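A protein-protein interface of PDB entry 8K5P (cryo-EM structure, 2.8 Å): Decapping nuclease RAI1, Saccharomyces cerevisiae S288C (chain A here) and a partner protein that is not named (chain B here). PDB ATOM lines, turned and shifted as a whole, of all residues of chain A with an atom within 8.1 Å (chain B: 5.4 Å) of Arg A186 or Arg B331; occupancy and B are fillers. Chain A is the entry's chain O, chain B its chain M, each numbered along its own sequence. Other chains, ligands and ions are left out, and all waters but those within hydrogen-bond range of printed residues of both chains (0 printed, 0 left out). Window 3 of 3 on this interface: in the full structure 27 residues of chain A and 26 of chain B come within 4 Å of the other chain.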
ATOM      1  N   TYR A  47     -12.752  -3.507  27.259  1.00  0.00           N
ATOM      2  CA  TYR A  47     -13.068  -4.789  27.886  1.00  0.00           C
ATOM      3  C   TYR A  47     -12.364  -4.844  29.231  1.00  0.00           C
ATOM      4  O   TYR A  47     -11.129  -4.835  29.280  1.00  0.00           O
ATOM      5  CB  TYR A  47     -12.637  -5.957  26.998  1.00  0.00           C
ATOM      6  CG  TYR A  47     -12.498  -7.269  27.737  1.00  0.00           C
ATOM      7  CD1 TYR A  47     -13.618  -7.971  28.161  1.00  0.00           C
ATOM      8  CD2 TYR A  47     -11.247  -7.804  28.012  1.00  0.00           C
ATOM      9  CE1 TYR A  47     -13.496  -9.170  28.837  1.00  0.00           C
ATOM     10  CE2 TYR A  47     -11.114  -9.001  28.686  1.00  0.00           C
ATOM     11  CZ  TYR A  47     -12.242  -9.680  29.096  1.00  0.00           C
ATOM     12  OH  TYR A  47     -12.112 -10.873  29.770  1.00  0.00           O
ATOM     13  N   ARG A  55      -8.329  -7.654  41.056  1.00  0.00           N
ATOM     14  CA  ARG A  55      -6.992  -8.239  41.044  1.00  0.00           C
ATOM     15  C   ARG A  55      -5.918  -7.280  41.543  1.00  0.00           C
ATOM     16  O   ARG A  55      -4.785  -7.719  41.770  1.00  0.00           O
ATOM     17  CB  ARG A  55      -6.643  -8.712  39.632  1.00  0.00           C
ATOM     18  CG  ARG A  55      -5.689  -9.895  39.587  1.00  0.00           C
ATOM     19  CD  ARG A  55      -5.901 -10.724  38.332  1.00  0.00           C
ATOM     20  NE  ARG A  55      -7.260 -11.244  38.245  1.00  0.00           N
ATOM     21  CZ  ARG A  55      -7.717 -11.981  37.242  1.00  0.00           C
ATOM     22  NH1 ARG A  55      -6.948 -12.305  36.216  1.00  0.00           N
ATOM     23  NH2 ARG A  55      -8.978 -12.403  37.270  1.00  0.00           N
ATOM     24  N   LEU A 177      -8.105  -3.820  23.973  1.00  0.00           N
ATOM     25  CA  LEU A 177      -7.406  -4.949  23.367  1.00  0.00           C
ATOM     26  C   LEU A 177      -7.341  -4.797  21.853  1.00  0.00           C
ATOM     27  O   LEU A 177      -7.389  -5.784  21.113  1.00  0.00           O
ATOM     28  CB  LEU A 177      -8.073  -6.270  23.749  1.00  0.00           C
ATOM     29  CG  LEU A 177      -7.604  -6.880  25.069  1.00  0.00           C
ATOM     30  CD1 LEU A 177      -8.636  -7.854  25.602  1.00  0.00           C
ATOM     31  CD2 LEU A 177      -6.258  -7.564  24.891  1.00  0.00           C
ATOM     32  N   LEU A 181     -12.943  -7.927  20.968  1.00  0.00           N
ATOM     33  CA  LEU A 181     -13.111  -9.214  21.617  1.00  0.00           C
ATOM     34  C   LEU A 181     -13.924 -10.134  20.709  1.00  0.00           C
ATOM     35  O   LEU A 181     -14.596  -9.686  19.774  1.00  0.00           O
ATOM     36  CB  LEU A 181     -13.792  -9.044  22.977  1.00  0.00           C
ATOM     37  CG  LEU A 181     -13.879 -10.256  23.910  1.00  0.00           C
ATOM     38  CD1 LEU A 181     -12.499 -10.853  24.150  1.00  0.00           C
ATOM     39  CD2 LEU A 181     -14.548  -9.888  25.225  1.00  0.00           C
ATOM     40  N   TYR A 183     -12.695 -12.103  18.627  1.00  0.00           N
ATOM     41  CA  TYR A 183     -11.882 -12.401  17.453  1.00  0.00           C
ATOM     42  C   TYR A 183     -10.391 -12.378  17.771  1.00  0.00           C
ATOM     43  O   TYR A 183      -9.573 -12.226  16.854  1.00  0.00           O
ATOM     44  CB  TYR A 183     -12.177 -11.419  16.314  1.00  0.00           C
ATOM     45  CG  TYR A 183     -13.632 -11.366  15.916  1.00  0.00           C
ATOM     46  CD1 TYR A 183     -14.179 -12.342  15.095  1.00  0.00           C
ATOM     47  CD2 TYR A 183     -14.458 -10.343  16.361  1.00  0.00           C
ATOM     48  CE1 TYR A 183     -15.507 -12.302  14.728  1.00  0.00           C
ATOM     49  CE2 TYR A 183     -15.791 -10.294  15.997  1.00  0.00           C
ATOM     50  CZ  TYR A 183     -16.309 -11.278  15.180  1.00  0.00           C
ATOM     51  OH  TYR A 183     -17.634 -11.239  14.813  1.00  0.00           O
ATOM     52  N   THR A 184     -10.015 -12.523  19.041  1.00  0.00           N
ATOM     53  CA  THR A 184      -8.624 -12.533  19.460  1.00  0.00           C
ATOM     54  C   THR A 184      -8.390 -13.739  20.359  1.00  0.00           C
ATOM     55  O   THR A 184      -9.285 -14.121  21.127  1.00  0.00           O
ATOM     56  CB  THR A 184      -8.246 -11.247  20.210  1.00  0.00           C
ATOM     57  OG1 THR A 184      -9.306 -10.886  21.104  1.00  0.00           O
ATOM     58  CG2 THR A 184      -8.004 -10.108  19.231  1.00  0.00           C
ATOM     59  N   PRO A 185      -7.214 -14.353  20.288  1.00  0.00           N
ATOM     60  CA  PRO A 185      -6.934 -15.518  21.134  1.00  0.00           C
ATOM     61  C   PRO A 185      -6.691 -15.106  22.579  1.00  0.00           C
ATOM     62  O   PRO A 185      -6.491 -13.934  22.905  1.00  0.00           O
ATOM     63  CB  PRO A 185      -5.673 -16.129  20.510  1.00  0.00           C
ATOM     64  CG  PRO A 185      -5.521 -15.456  19.169  1.00  0.00           C
ATOM     65  CD  PRO A 185      -6.127 -14.101  19.329  1.00  0.00           C
ATOM     66  N   ARG A 186      -6.713 -16.110  23.459  1.00  0.00           N
ATOM     67  CA  ARG A 186      -6.442 -15.877  24.873  1.00  0.00           C
ATOM     68  C   ARG A 186      -5.004 -15.436  25.116  1.00  0.00           C
ATOM     69  O   ARG A 186      -4.719 -14.827  26.155  1.00  0.00           O
ATOM     70  CB  ARG A 186      -6.754 -17.140  25.678  1.00  0.00           C
ATOM     71  CG  ARG A 186      -6.769 -16.944  27.186  1.00  0.00           C
ATOM     72  CD  ARG A 186      -7.073 -18.245  27.909  1.00  0.00           C
ATOM     73  NE  ARG A 186      -8.465 -18.648  27.741  1.00  0.00           N
ATOM     74  CZ  ARG A 186      -9.448 -18.308  28.563  1.00  0.00           C
ATOM     75  NH1 ARG A 186      -9.229 -17.553  29.627  1.00  0.00           N
ATOM     76  NH2 ARG A 186     -10.682 -18.735  28.311  1.00  0.00           N
ATOM     77  N   GLU A 187      -4.097 -15.726  24.178  1.00  0.00           N
ATOM     78  CA  GLU A 187      -2.713 -15.289  24.325  1.00  0.00           C
ATOM     79  C   GLU A 187      -2.619 -13.770  24.371  1.00  0.00           C
ATOM     80  O   GLU A 187      -1.863 -13.213  25.175  1.00  0.00           O
ATOM     81  CB  GLU A 187      -1.864 -15.846  23.182  1.00  0.00           C
ATOM     82  CG  GLU A 187      -0.368 -15.669  23.379  1.00  0.00           C
ATOM     83  CD  GLU A 187       0.214 -16.674  24.354  1.00  0.00           C
ATOM     84  OE1 GLU A 187      -0.435 -17.714  24.595  1.00  0.00           O
ATOM     85  OE2 GLU A 187       1.319 -16.424  24.878  1.00  0.00           O
ATOM     86  N   VAL A 188      -3.384 -13.080  23.523  1.00  0.00           N
ATOM     87  CA  VAL A 188      -3.402 -11.621  23.561  1.00  0.00           C
ATOM     88  C   VAL A 188      -3.978 -11.131  24.883  1.00  0.00           C
ATOM     89  O   VAL A 188      -3.502 -10.145  25.460  1.00  0.00           O
ATOM     90  CB  VAL A 188      -4.186 -11.063  22.359  1.00  0.00           C
ATOM     91  CG1 VAL A 188      -3.952  -9.566  22.222  1.00  0.00           C
ATOM     92  CG2 VAL A 188      -3.787 -11.790  21.084  1.00  0.00           C
ATOM     93  N   ILE A 189      -5.010 -11.815  25.386  1.00  0.00           N
ATOM     94  CA  ILE A 189      -5.631 -11.411  26.645  1.00  0.00           C
ATOM     95  C   ILE A 189      -4.630 -11.502  27.789  1.00  0.00           C
ATOM     96  O   ILE A 189      -4.538 -10.595  28.626  1.00  0.00           O
ATOM     97  CB  ILE A 189      -6.883 -12.264  26.923  1.00  0.00           C
ATOM     98  CG1 ILE A 189      -7.630 -12.565  25.622  1.00  0.00           C
ATOM     99  CG2 ILE A 189      -7.795 -11.562  27.919  1.00  0.00           C
ATOM    100  CD1 ILE A 189      -8.397 -11.394  25.061  1.00  0.00           C
ATOM    101  N   GLU A 190      -3.864 -12.593  27.847  1.00  0.00           N
ATOM    102  CA  GLU A 190      -2.886 -12.736  28.921  1.00  0.00           C
ATOM    103  C   GLU A 190      -1.665 -11.848  28.710  1.00  0.00           C
ATOM    104  O   GLU A 190      -1.029 -11.439  29.687  1.00  0.00           O
ATOM    105  CB  GLU A 190      -2.465 -14.202  29.067  1.00  0.00           C
ATOM    106  CG  GLU A 190      -1.746 -14.789  27.864  1.00  0.00           C
ATOM    107  CD  GLU A 190      -0.237 -14.703  27.986  1.00  0.00           C
ATOM    108  OE1 GLU A 190       0.278 -14.827  29.118  1.00  0.00           O
ATOM    109  OE2 GLU A 190       0.435 -14.514  26.951  1.00  0.00           O
ATOM    110  N   LYS A 191      -1.322 -11.538  27.457  1.00  0.00           N
ATOM    111  CA  LYS A 191      -0.198 -10.656  27.171  1.00  0.00           C
ATOM    112  C   LYS A 191      -0.521  -9.191  27.436  1.00  0.00           C
ATOM    113  O   LYS A 191       0.400  -8.397  27.658  1.00  0.00           O
ATOM    114  CB  LYS A 191       0.244 -10.840  25.716  1.00  0.00           C
ATOM    115  CG  LYS A 191       1.494 -10.068  25.318  1.00  0.00           C
ATOM    116  CD  LYS A 191       1.161  -8.955  24.337  1.00  0.00           C
ATOM    117  CE  LYS A 191       2.375  -8.086  24.052  1.00  0.00           C
ATOM    118  NZ  LYS A 191       2.023  -6.900  23.222  1.00  0.00           N
ATOM    119  N   ARG A 192      -1.806  -8.820  27.427  1.00  0.00           N
ATOM    120  CA  ARG A 192      -2.177  -7.423  27.638  1.00  0.00           C
ATOM    121  C   ARG A 192      -1.679  -6.893  28.978  1.00  0.00           C
ATOM    122  O   ARG A 192      -1.474  -5.682  29.125  1.00  0.00           O
ATOM    123  CB  ARG A 192      -3.696  -7.264  27.532  1.00  0.00           C
ATOM    124  CG  ARG A 192      -4.421  -7.218  28.869  1.00  0.00           C
ATOM    125  CD  ARG A 192      -5.920  -7.391  28.697  1.00  0.00           C
ATOM    126  NE  ARG A 192      -6.557  -6.178  28.200  1.00  0.00           N
ATOM    127  CZ  ARG A 192      -7.789  -5.800  28.510  1.00  0.00           C
ATOM    128  NH1 ARG A 192      -8.549  -6.517  29.321  1.00  0.00           N
ATOM    129  NH2 ARG A 192      -8.271  -4.674  27.993  1.00  0.00           N
ATOM    130  N   HIS B 257     -20.873 -20.503  30.628  1.00  0.00           N
ATOM    131  CA  HIS B 257     -20.381 -19.223  31.144  1.00  0.00           C
ATOM    132  C   HIS B 257     -21.389 -18.101  30.908  1.00  0.00           C
ATOM    133  O   HIS B 257     -21.022 -16.968  30.587  1.00  0.00           O
ATOM    134  CB  HIS B 257     -19.018 -18.871  30.543  1.00  0.00           C
ATOM    135  CG  HIS B 257     -17.918 -19.796  30.961  1.00  0.00           C
ATOM    136  ND1 HIS B 257     -17.789 -21.072  30.459  1.00  0.00           N
ATOM    137  CD2 HIS B 257     -16.899 -19.630  31.837  1.00  0.00           C
ATOM    138  CE1 HIS B 257     -16.735 -21.653  31.006  1.00  0.00           C
ATOM    139  NE2 HIS B 257     -16.178 -20.800  31.846  1.00  0.00           N
ATOM    140  N   ASP B 328      -9.069 -16.980  38.723  1.00  0.00           N
ATOM    141  CA  ASP B 328     -10.121 -16.521  37.827  1.00  0.00           C
ATOM    142  C   ASP B 328     -11.356 -17.387  38.024  1.00  0.00           C
ATOM    143  O   ASP B 328     -11.261 -18.619  38.019  1.00  0.00           O
ATOM    144  CB  ASP B 328      -9.664 -16.576  36.367  1.00  0.00           C
ATOM    145  CG  ASP B 328      -8.329 -15.894  36.147  1.00  0.00           C
ATOM    146  OD1 ASP B 328      -7.940 -15.055  36.986  1.00  0.00           O
ATOM    147  OD2 ASP B 328      -7.666 -16.196  35.132  1.00  0.00           O
ATOM    148  N   LEU B 329     -12.511 -16.741  38.201  1.00  0.00           N
ATOM    149  CA  LEU B 329     -13.750 -17.486  38.397  1.00  0.00           C
ATOM    150  C   LEU B 329     -14.106 -18.302  37.161  1.00  0.00           C
ATOM    151  O   LEU B 329     -14.548 -19.452  37.274  1.00  0.00           O
ATOM    152  CB  LEU B 329     -14.886 -16.530  38.758  1.00  0.00           C
ATOM    153  CG  LEU B 329     -16.115 -17.127  39.452  1.00  0.00           C
ATOM    154  CD1 LEU B 329     -17.251 -17.319  38.460  1.00  0.00           C
ATOM    155  CD2 LEU B 329     -15.779 -18.439  40.149  1.00  0.00           C
ATOM    156  N   GLU B 330     -13.925 -17.724  35.971  1.00  0.00           N
ATOM    157  CA  GLU B 330     -14.247 -18.445  34.743  1.00  0.00           C
ATOM    158  C   GLU B 330     -13.374 -19.683  34.583  1.00  0.00           C
ATOM    159  O   GLU B 330     -13.862 -20.749  34.191  1.00  0.00           O
ATOM    160  CB  GLU B 330     -14.095 -17.517  33.538  1.00  0.00           C
ATOM    161  CG  GLU B 330     -15.110 -16.385  33.504  1.00  0.00           C
ATOM    162  CD  GLU B 330     -15.172 -15.698  32.156  1.00  0.00           C
ATOM    163  OE1 GLU B 330     -14.315 -14.828  31.893  1.00  0.00           O
ATOM    164  OE2 GLU B 330     -16.076 -16.027  31.360  1.00  0.00           O
ATOM    165  N   ARG B 331     -12.078 -19.562  34.881  1.00  0.00           N
ATOM    166  CA  ARG B 331     -11.191 -20.716  34.810  1.00  0.00           C
ATOM    167  C   ARG B 331     -11.404 -21.681  35.968  1.00  0.00           C
ATOM    168  O   ARG B 331     -11.107 -22.872  35.828  1.00  0.00           O
ATOM    169  CB  ARG B 331      -9.732 -20.258  34.779  1.00  0.00           C
ATOM    170  CG  ARG B 331      -9.450 -19.151  33.778  1.00  0.00           C
ATOM    171  CD  ARG B 331      -9.018 -19.719  32.438  1.00  0.00           C
ATOM    172  NE  ARG B 331      -7.912 -20.659  32.577  1.00  0.00           N
ATOM    173  CZ  ARG B 331      -7.247 -21.189  31.560  1.00  0.00           C
ATOM    174  NH1 ARG B 331      -7.547 -20.887  30.307  1.00  0.00           N
ATOM    175  NH2 ARG B 331      -6.257 -22.041  31.805  1.00  0.00           N
ATOM    176  N   ALA B 332     -11.904 -21.196  37.107  1.00  0.00           N
ATOM    177  CA  ALA B 332     -12.152 -22.078  38.244  1.00  0.00           C
ATOM    178  C   ALA B 332     -13.239 -23.097  37.929  1.00  0.00           C
ATOM    179  O   ALA B 332     -13.146 -24.260  38.336  1.00  0.00           O
ATOM    180  CB  ALA B 332     -12.526 -21.256  39.477  1.00  0.00           C
ATOM    181  N   ILE B 333     -14.284 -22.678  37.211  1.00  0.00           N
ATOM    182  CA  ILE B 333     -15.363 -23.594  36.868  1.00  0.00           C
ATOM    183  C   ILE B 333     -14.914 -24.646  35.860  1.00  0.00           C
ATOM    184  O   ILE B 333     -15.487 -25.740  35.817  1.00  0.00           O
ATOM    185  CB  ILE B 333     -16.576 -22.809  36.335  1.00  0.00           C
ATOM    186  CG1 ILE B 333     -16.882 -21.618  37.248  1.00  0.00           C
ATOM    187  CG2 ILE B 333     -17.790 -23.714  36.205  1.00  0.00           C
ATOM    188  CD1 ILE B 333     -17.861 -21.924  38.361  1.00  0.00           C
ATOM    189  N   ASP B 334     -13.898 -24.345  35.047  1.00  0.00           N
ATOM    190  CA  ASP B 334     -13.470 -25.283  34.012  1.00  0.00           C
ATOM    191  C   ASP B 334     -12.941 -26.578  34.619  1.00  0.00           C
ATOM    192  O   ASP B 334     -13.303 -27.676  34.178  1.00  0.00           O
ATOM    193  CB  ASP B 334     -12.413 -24.629  33.124  1.00  0.00           C
ATOM    194  CG  ASP B 334     -12.939 -23.408  32.394  1.00  0.00           C
ATOM    195  OD1 ASP B 334     -14.168 -23.317  32.195  1.00  0.00           O
ATOM    196  OD2 ASP B 334     -12.123 -22.540  32.020  1.00  0.00           O
ATOM    197  N   ASP B 335     -12.084 -26.471  35.637  1.00  0.00           N
ATOM    198  CA  ASP B 335     -11.575 -27.673  36.287  1.00  0.00           C
ATOM    199  C   ASP B 335     -12.697 -28.439  36.974  1.00  0.00           C
ATOM    200  O   ASP B 335     -12.720 -29.673  36.951  1.00  0.00           O
ATOM    201  CB  ASP B 335     -10.475 -27.315  37.285  1.00  0.00           C
ATOM    202  CG  ASP B 335     -10.892 -26.226  38.249  1.00  0.00           C
ATOM    203  OD1 ASP B 335     -11.653 -26.524  39.192  1.00  0.00           O
ATOM    204  OD2 ASP B 335     -10.451 -25.071  38.068  1.00  0.00           O
ATOM    205  N   TYR B 378      -3.160 -23.671  35.433  1.00  0.00           N
ATOM    206  CA  TYR B 378      -4.530 -24.117  35.628  1.00  0.00           C
ATOM    207  C   TYR B 378      -4.721 -25.528  35.072  1.00  0.00           C
ATOM    208  O   TYR B 378      -3.876 -26.071  34.355  1.00  0.00           O
ATOM    209  CB  TYR B 378      -5.508 -23.150  34.966  1.00  0.00           C
ATOM    210  CG  TYR B 378      -6.159 -22.184  35.929  1.00  0.00           C
ATOM    211  CD1 TYR B 378      -7.030 -22.635  36.913  1.00  0.00           C
ATOM    212  CD2 TYR B 378      -5.904 -20.821  35.855  1.00  0.00           C
ATOM    213  CE1 TYR B 378      -7.627 -21.755  37.796  1.00  0.00           C
ATOM    214  CE2 TYR B 378      -6.496 -19.935  36.733  1.00  0.00           C
ATOM    215  CZ  TYR B 378      -7.357 -20.407  37.701  1.00  0.00           C
ATOM    216  OH  TYR B 378      -7.949 -19.527  38.577  1.00  0.00           O
ATOM    217  N   THR B 380      -7.374 -26.803  32.966  1.00  0.00           N
ATOM    218  CA  THR B 380      -7.722 -26.817  31.555  1.00  0.00           C
ATOM    219  C   THR B 380      -7.691 -25.402  30.994  1.00  0.00           C
ATOM    220  O   THR B 380      -7.948 -24.426  31.708  1.00  0.00           O
ATOM    221  CB  THR B 380      -9.111 -27.429  31.323  1.00  0.00           C
ATOM    222  OG1 THR B 380     -10.114 -26.568  31.876  1.00  0.00           O
ATOM    223  CG2 THR B 380      -9.210 -28.798  31.978  1.00  0.00           C
ATOM    224  N   CYS B 381      -7.375 -25.299  29.706  1.00  0.00           N
ATOM    225  CA  CYS B 381      -7.310 -24.022  28.997  1.00  0.00           C
ATOM    226  C   CYS B 381      -8.275 -24.084  27.817  1.00  0.00           C
ATOM    227  O   CYS B 381      -7.918 -24.579  26.742  1.00  0.00           O
ATOM    228  CB  CYS B 381      -5.886 -23.722  28.538  1.00  0.00           C
ATOM    229  SG  CYS B 381      -5.544 -21.967  28.272  1.00  0.00           S
ATOM    230  N   ASP B 382      -9.492 -23.576  28.025  1.00  0.00           N
ATOM    231  CA  ASP B 382     -10.530 -23.547  26.992  1.00  0.00           C
ATOM    232  C   ASP B 382     -10.804 -24.941  26.430  1.00  0.00           C
ATOM    233  O   ASP B 382     -10.968 -25.124  25.223  1.00  0.00           O
ATOM    234  CB  ASP B 382     -10.166 -22.572  25.870  1.00  0.00           C
ATOM    235  CG  ASP B 382     -11.384 -22.049  25.139  1.00  0.00           C
ATOM    236  OD1 ASP B 382     -12.480 -22.048  25.739  1.00  0.00           O
ATOM    237  OD2 ASP B 382     -11.248 -21.643  23.965  1.00  0.00           O
ATOM    238  N   LYS B 871     -13.867 -19.224  23.327  1.00  0.00           N
ATOM    239  CA  LYS B 871     -13.216 -19.042  24.612  1.00  0.00           C
ATOM    240  C   LYS B 871     -14.254 -18.878  25.720  1.00  0.00           C
ATOM    241  O   LYS B 871     -15.457 -18.759  25.475  1.00  0.00           O
ATOM    242  CB  LYS B 871     -12.282 -17.833  24.574  1.00  0.00           C
ATOM    243  CG  LYS B 871     -11.535 -17.666  23.261  1.00  0.00           C
ATOM    244  CD  LYS B 871     -10.878 -16.298  23.173  1.00  0.00           C
ATOM    245  CE  LYS B 871     -11.885 -15.183  23.401  1.00  0.00           C
ATOM    246  NZ  LYS B 871     -12.998 -15.229  22.414  1.00  0.00           N
ATOM    247  N   SER B 872     -13.770 -18.872  26.959  1.00  0.00           N
ATOM    248  CA  SER B 872     -14.608 -18.683  28.140  1.00  0.00           C
ATOM    249  C   SER B 872     -14.272 -17.313  28.723  1.00  0.00           C
ATOM    250  O   SER B 872     -13.442 -17.189  29.625  1.00  0.00           O
ATOM    251  CB  SER B 872     -14.385 -19.799  29.156  1.00  0.00           C
ATOM    252  OG  SER B 872     -13.009 -19.943  29.462  1.00  0.00           O
ATOM    253  N   ILE B 873     -14.928 -16.281  28.198  1.00  0.00           N
ATOM    254  CA  ILE B 873     -14.703 -14.903  28.617  1.00  0.00           C
ATOM    255  C   ILE B 873     -16.053 -14.216  28.746  1.00  0.00           C
ATOM    256  O   ILE B 873     -16.895 -14.317  27.847  1.00  0.00           O
ATOM    257  CB  ILE B 873     -13.796 -14.146  27.624  1.00  0.00           C
ATOM    258  CG1 ILE B 873     -12.333 -14.547  27.826  1.00  0.00           C
ATOM    259  CG2 ILE B 873     -13.967 -12.642  27.769  1.00  0.00           C
ATOM    260  CD1 ILE B 873     -11.810 -14.268  29.218  1.00  0.00           C
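The side-chain hydroxyl (OG) of Ser B872 lies within hydrogen-bond range of the guanidinium group (NH2) of Arg A186, at 2.9 Å. The side-chain carboxylate (OD1) of Asp B328 is in salt-bridge range of the guanidinium group (NH2) of Arg A55, 2.9 Å away.
The side-chain carboxylate (OE2) of Glu B330 lies close to the backbone NH (N) of Ile B873 (3.4 Å). The side-chain hydroxyl of Tyr B378 lies within hydrogen-bond range of the backbone NH of Asp B328 (2.8 Å). The backbone carbonyl oxygen (O) of Tyr A47 lies within hydrogen-bond range of the guanidinium group (NH1) of Arg A192 (3.1 Å). The side-chain sulfur of Cys B381 sits at hydrogen-bond distance from the guanidinium group of Arg B331 (3.1 Å). The backbone carbonyl oxygen of Thr B380 is in hydrogen-bond range of the guanidinium group of Arg B331, at 2.9 Å.
Among the printed residues, pairs that only touch across the chains: Tyr A47 with Ile B873 (3.3 Å), Thr A184 with Lys B871 (3.4 Å), Arg A186 with Arg B331 (3.5 Å) and Leu A181 with Ile B873 (3.8 Å).
Printed residues of chain B within 4 Å of Tyr A47: Ile B873. Of the printed residues of chain B, Arg A55 touches Asp B328 (2.9 Å). Of the printed residues of chain B, Leu A181 touches Ile B873. Arg A186 touches just these residues of chain B: Arg B331 (3.5 Å) and Ser B872 (2.9 Å). Of the printed residues of chain A, Asp B328 touches Arg A55. Of chain A, only Arg A186 comes within 4 Å of Arg B331. Ala B332 touches none of the printed residues of chain A. Ile B333 touches none of the printed residues of chain A. Cys B381 touches none of the printed residues of chain A. The nearest residue of chain A that does not touch Arg B331 is Arg A55 (7.6 Å). The nearest printed residue of chain B that does not touch Thr A184 is Ile B873 (7.4 Å).
Of the 16 printed residues of chain B, 5 touch a printed residue of chain A. Hydrophobic or aromatic side chains of chain B that line the printed part of chain A: Ile B873. Hydrophobic or aromatic side chains of chain A within 4 Å of the printed part of chain B: Tyr A47 and Leu A181. Among the printed residues, 6 pairs touch across the chains.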
